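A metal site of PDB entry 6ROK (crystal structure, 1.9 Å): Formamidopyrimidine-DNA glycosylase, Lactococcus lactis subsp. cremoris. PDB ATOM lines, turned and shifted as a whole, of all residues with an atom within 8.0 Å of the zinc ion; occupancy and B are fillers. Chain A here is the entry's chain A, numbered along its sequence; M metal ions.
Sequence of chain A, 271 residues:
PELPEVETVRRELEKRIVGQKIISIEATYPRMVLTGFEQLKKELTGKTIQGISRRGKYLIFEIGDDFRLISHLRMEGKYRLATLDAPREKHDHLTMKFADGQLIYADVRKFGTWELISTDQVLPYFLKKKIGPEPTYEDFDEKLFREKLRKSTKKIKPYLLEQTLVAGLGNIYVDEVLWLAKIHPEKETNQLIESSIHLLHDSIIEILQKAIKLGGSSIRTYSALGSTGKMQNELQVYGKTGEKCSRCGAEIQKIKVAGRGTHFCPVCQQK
SG of Cys 265 is bound to the zinc ion, at 2.1 Å.
The side-chain sulfur (SG) of Cys 268 is bound to the zinc ion (2.3 Å).
The zinc ion is bound by SG of Cys 248 (2.4 Å).
The zinc ion is bound by SG of Cys 245, 2.4 Å away.
Within 4 Å of the zinc ion: Cys 245, Cys 248, Cys 265 and Cys 268.
Along chain A the residues within 4 Å of the zinc ion span positions 245 to 268.
SG of Cys 265 lies close to N of Val 267, at 3.5 Å.
N of Cys 265 sits at hydrogen-bond distance from OE1 of Gln 269 (2.8 Å).
NE of Arg 247 lies close to SG of Cys 268 (3.4 Å).
The backbone NH (N) of Ala 250 lies close to the side-chain sulfur (SG) of Cys 248 (3.3 Å).
The side-chain sulfur (SG) of Cys 245 lies close to the indole nitrogen (NE1) of Trp 179, at 3.4 Å.
The side-chain sulfur (SG) of Cys 245 lies close to the backbone NH (N) of Arg 247.
N of Cys 245 lies within hydrogen-bond range of O of Ala 250 (2.7 Å).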
ATOM      1  N   TRP A 179      24.942  -8.890  20.605  1.00  0.00           N
ATOM      2  CA  TRP A 179      25.589  -7.663  20.166  1.00  0.00           C
ATOM      3  C   TRP A 179      27.091  -7.893  19.981  1.00  0.00           C
ATOM      4  O   TRP A 179      27.696  -7.475  18.968  1.00  0.00           O
ATOM      5  CB  TRP A 179      25.308  -6.529  21.178  1.00  0.00           C
ATOM      6  CG  TRP A 179      26.019  -5.238  20.824  1.00  0.00           C
ATOM      7  CD1 TRP A 179      25.552  -4.212  19.997  1.00  0.00           C
ATOM      8  CD2 TRP A 179      27.333  -4.837  21.238  1.00  0.00           C
ATOM      9  NE1 TRP A 179      26.467  -3.211  19.953  1.00  0.00           N
ATOM     10  CE2 TRP A 179      27.581  -3.567  20.654  1.00  0.00           C
ATOM     11  CE3 TRP A 179      28.319  -5.420  22.042  1.00  0.00           C
ATOM     12  CZ2 TRP A 179      28.773  -2.870  20.848  1.00  0.00           C
ATOM     13  CZ3 TRP A 179      29.510  -4.724  22.236  1.00  0.00           C
ATOM     14  CH2 TRP A 179      29.729  -3.465  21.624  1.00  0.00           C
ATOM     15  N   LYS A 182      27.773  -9.817  16.937  1.00  0.00           N
ATOM     16  CA  LYS A 182      27.264  -9.156  15.729  1.00  0.00           C
ATOM     17  C   LYS A 182      26.228 -10.025  15.026  1.00  0.00           C
ATOM     18  O   LYS A 182      26.218 -10.194  13.797  1.00  0.00           O
ATOM     19  CB  LYS A 182      28.418  -8.772  14.793  1.00  0.00           C
ATOM     20  CG  LYS A 182      29.322  -7.684  15.421  1.00  0.00           C
ATOM     21  CD  LYS A 182      30.484  -7.376  14.469  1.00  0.00           C
ATOM     22  CE  LYS A 182      31.495  -6.389  15.134  1.00  0.00           C
ATOM     23  NZ  LYS A 182      32.468  -5.696  14.173  1.00  0.00           N
ATOM     24  N   VAL A 237      24.101  -3.107  25.365  1.00  0.00           N
ATOM     25  CA  VAL A 237      22.796  -2.933  24.721  1.00  0.00           C
ATOM     26  C   VAL A 237      21.618  -3.103  25.703  1.00  0.00           C
ATOM     27  O   VAL A 237      20.586  -2.439  25.549  1.00  0.00           O
ATOM     28  CB  VAL A 237      22.626  -3.895  23.542  1.00  0.00           C
ATOM     29  CG1 VAL A 237      23.539  -3.504  22.411  1.00  0.00           C
ATOM     30  CG2 VAL A 237      22.945  -5.366  23.965  1.00  0.00           C
ATOM     31  N   LYS A 244      23.474   5.384  22.079  1.00  0.00           N
ATOM     32  CA  LYS A 244      24.321   5.146  20.931  1.00  0.00           C
ATOM     33  C   LYS A 244      25.132   3.877  21.144  1.00  0.00           C
ATOM     34  O   LYS A 244      25.701   3.680  22.224  1.00  0.00           O
ATOM     35  CB  LYS A 244      25.240   6.350  20.710  1.00  0.00           C
ATOM     36  CG  LYS A 244      24.705   7.441  19.800  1.00  0.00           C
ATOM     37  CD  LYS A 244      23.177   7.568  19.728  1.00  0.00           C
ATOM     38  CE  LYS A 244      22.768   9.036  19.349  1.00  0.00           C
ATOM     39  NZ  LYS A 244      21.458   9.169  18.583  1.00  0.00           N
ATOM     40  N   CYS A 245      25.128   2.977  20.145  1.00  0.00           N
ATOM     41  CA  CYS A 245      26.054   1.832  20.122  1.00  0.00           C
ATOM     42  C   CYS A 245      27.497   2.291  20.264  1.00  0.00           C
ATOM     43  O   CYS A 245      27.937   3.208  19.564  1.00  0.00           O
ATOM     44  CB  CYS A 245      25.902   1.084  18.799  1.00  0.00           C
ATOM     45  SG  CYS A 245      27.110  -0.260  18.503  1.00  0.00           S
ATOM     46  N   SER A 246      28.274   1.614  21.107  1.00  0.00           N
ATOM     47  CA  SER A 246      29.662   2.061  21.265  1.00  0.00           C
ATOM     48  C   SER A 246      30.573   1.700  20.093  1.00  0.00           C
ATOM     49  O   SER A 246      31.695   2.226  20.046  1.00  0.00           O
ATOM     50  CB  SER A 246      30.256   1.472  22.550  1.00  0.00           C
ATOM     51  OG  SER A 246      30.148   0.058  22.506  1.00  0.00           O
ATOM     52  N   ARG A 247      30.156   0.850  19.154  1.00  0.00           N
ATOM     53  CA  ARG A 247      31.014   0.512  18.015  1.00  0.00           C
ATOM     54  C   ARG A 247      30.747   1.438  16.835  1.00  0.00           C
ATOM     55  O   ARG A 247      31.683   1.978  16.248  1.00  0.00           O
ATOM     56  CB  ARG A 247      30.825  -0.944  17.567  1.00  0.00           C
ATOM     57  CG  ARG A 247      31.579  -1.925  18.430  1.00  0.00           C
ATOM     58  CD  ARG A 247      31.447  -3.394  17.943  1.00  0.00           C
ATOM     59  NE  ARG A 247      30.042  -3.764  17.794  1.00  0.00           N
ATOM     60  CZ  ARG A 247      29.529  -4.951  18.093  1.00  0.00           C
ATOM     61  NH1 ARG A 247      30.314  -5.896  18.595  1.00  0.00           N
ATOM     62  NH2 ARG A 247      28.233  -5.191  17.919  1.00  0.00           N
ATOM     63  N   CYS A 248      29.486   1.644  16.499  1.00  0.00           N
ATOM     64  CA  CYS A 248      29.146   2.322  15.278  1.00  0.00           C
ATOM     65  C   CYS A 248      28.332   3.578  15.472  1.00  0.00           C
ATOM     66  O   CYS A 248      28.120   4.280  14.488  1.00  0.00           O
ATOM     67  CB  CYS A 248      28.344   1.378  14.369  1.00  0.00           C
ATOM     68  SG  CYS A 248      26.662   1.258  14.910  1.00  0.00           S
ATOM     69  N   GLY A 249      27.801   3.858  16.683  1.00  0.00           N
ATOM     70  CA  GLY A 249      27.089   5.095  16.895  1.00  0.00           C
ATOM     71  C   GLY A 249      25.613   5.072  16.532  1.00  0.00           C
ATOM     72  O   GLY A 249      24.919   6.071  16.765  1.00  0.00           O
ATOM     73  N   ALA A 250      25.110   3.990  15.956  1.00  0.00           N
ATOM     74  CA  ALA A 250      23.672   3.936  15.732  1.00  0.00           C
ATOM     75  C   ALA A 250      22.947   3.803  17.079  1.00  0.00           C
ATOM     76  O   ALA A 250      23.518   3.314  18.042  1.00  0.00           O
ATOM     77  CB  ALA A 250      23.327   2.766  14.807  1.00  0.00           C
ATOM     78  N   GLU A 251      21.679   4.263  17.129  1.00  0.00           N
ATOM     79  CA  GLU A 251      20.870   4.087  18.339  1.00  0.00           C
ATOM     80  C   GLU A 251      20.481   2.630  18.564  1.00  0.00           C
ATOM     81  O   GLU A 251      20.011   1.954  17.639  1.00  0.00           O
ATOM     82  CB  GLU A 251      19.573   4.901  18.296  1.00  0.00           C
ATOM     83  CG  GLU A 251      19.776   6.363  18.495  1.00  0.00           C
ATOM     84  CD  GLU A 251      18.496   7.112  18.830  1.00  0.00           C
ATOM     85  OE1 GLU A 251      17.410   6.487  18.936  1.00  0.00           O
ATOM     86  OE2 GLU A 251      18.592   8.337  18.999  1.00  0.00           O
ATOM     87  N   ILE A 252      20.589   2.165  19.813  1.00  0.00           N
ATOM     88  CA  ILE A 252      20.094   0.843  20.158  1.00  0.00           C
ATOM     89  C   ILE A 252      18.571   0.828  20.037  1.00  0.00           C
ATOM     90  O   ILE A 252      17.897   1.761  20.444  1.00  0.00           O
ATOM     91  CB  ILE A 252      20.545   0.457  21.582  1.00  0.00           C
ATOM     92  CG1 ILE A 252      22.076   0.549  21.714  1.00  0.00           C
ATOM     93  CG2 ILE A 252      19.998  -0.930  21.966  1.00  0.00           C
ATOM     94  CD1 ILE A 252      22.854  -0.156  20.564  1.00  0.00           C
ATOM     95  N   PHE A 264      19.220  -4.312  20.606  1.00  0.00           N
ATOM     96  CA  PHE A 264      20.251  -4.667  19.649  1.00  0.00           C
ATOM     97  C   PHE A 264      20.631  -3.424  18.844  1.00  0.00           C
ATOM     98  O   PHE A 264      19.837  -2.490  18.726  1.00  0.00           O
ATOM     99  CB  PHE A 264      19.783  -5.797  18.702  1.00  0.00           C
ATOM    100  CG  PHE A 264      18.740  -5.313  17.709  1.00  0.00           C
ATOM    101  CD1 PHE A 264      17.453  -4.987  18.160  1.00  0.00           C
ATOM    102  CD2 PHE A 264      19.066  -5.087  16.376  1.00  0.00           C
ATOM    103  CE1 PHE A 264      16.497  -4.485  17.282  1.00  0.00           C
ATOM    104  CE2 PHE A 264      18.100  -4.590  15.480  1.00  0.00           C
ATOM    105  CZ  PHE A 264      16.804  -4.294  15.937  1.00  0.00           C
ATOM    106  N   CYS A 265      21.835  -3.456  18.252  1.00  0.00           N
ATOM    107  CA  CYS A 265      22.263  -2.431  17.280  1.00  0.00           C
ATOM    108  C   CYS A 265      21.844  -2.868  15.878  1.00  0.00           C
ATOM    109  O   CYS A 265      22.322  -3.887  15.402  1.00  0.00           O
ATOM    110  CB  CYS A 265      23.776  -2.222  17.334  1.00  0.00           C
ATOM    111  SG  CYS A 265      24.444  -1.020  16.044  1.00  0.00           S
ATOM    112  N   PRO A 266      20.960  -2.133  15.198  1.00  0.00           N
ATOM    113  CA  PRO A 266      20.552  -2.517  13.834  1.00  0.00           C
ATOM    114  C   PRO A 266      21.662  -2.435  12.787  1.00  0.00           C
ATOM    115  O   PRO A 266      21.498  -2.987  11.695  1.00  0.00           O
ATOM    116  CB  PRO A 266      19.418  -1.520  13.502  1.00  0.00           C
ATOM    117  CG  PRO A 266      19.300  -0.605  14.662  1.00  0.00           C
ATOM    118  CD  PRO A 266      20.415  -0.831  15.621  1.00  0.00           C
ATOM    119  N   VAL A 267      22.753  -1.715  13.040  1.00  0.00           N
ATOM    120  CA  VAL A 267      23.875  -1.682  12.099  1.00  0.00           C
ATOM    121  C   VAL A 267      24.784  -2.883  12.325  1.00  0.00           C
ATOM    122  O   VAL A 267      25.081  -3.650  11.400  1.00  0.00           O
ATOM    123  CB  VAL A 267      24.655  -0.369  12.286  1.00  0.00           C
ATOM    124  CG1 VAL A 267      25.969  -0.407  11.516  1.00  0.00           C
ATOM    125  CG2 VAL A 267      23.788   0.816  11.823  1.00  0.00           C
ATOM    126  N   CYS A 268      25.240  -3.050  13.557  1.00  0.00           N
ATOM    127  CA  CYS A 268      26.156  -4.113  13.925  1.00  0.00           C
ATOM    128  C   CYS A 268      25.519  -5.503  13.828  1.00  0.00           C
ATOM    129  O   CYS A 268      26.217  -6.506  13.682  1.00  0.00           O
ATOM    130  CB  CYS A 268      26.632  -3.872  15.369  1.00  0.00           C
ATOM    131  SG  CYS A 268      27.824  -2.471  15.586  1.00  0.00           S
ATOM    132  N   GLN A 269      24.196  -5.588  13.978  1.00  0.00           N
ATOM    133  CA  GLN A 269      23.502  -6.868  14.002  1.00  0.00           C
ATOM    134  C   GLN A 269      22.502  -6.899  12.870  1.00  0.00           C
ATOM    135  O   GLN A 269      21.301  -6.642  13.073  1.00  0.00           O
ATOM    136  CB  GLN A 269      22.837  -7.087  15.318  1.00  0.00           C
ATOM    137  CG  GLN A 269      23.872  -7.263  16.453  1.00  0.00           C
ATOM    138  CD  GLN A 269      23.198  -7.054  17.829  1.00  0.00           C
ATOM    139  OE1 GLN A 269      23.192  -5.954  18.404  1.00  0.00           O
ATOM    140  NE2 GLN A 269      22.608  -8.126  18.353  1.00  0.00           N
HETATM  141 ZN    ZN M   1      26.528  -0.709  16.237  1.00  0.00          ZN
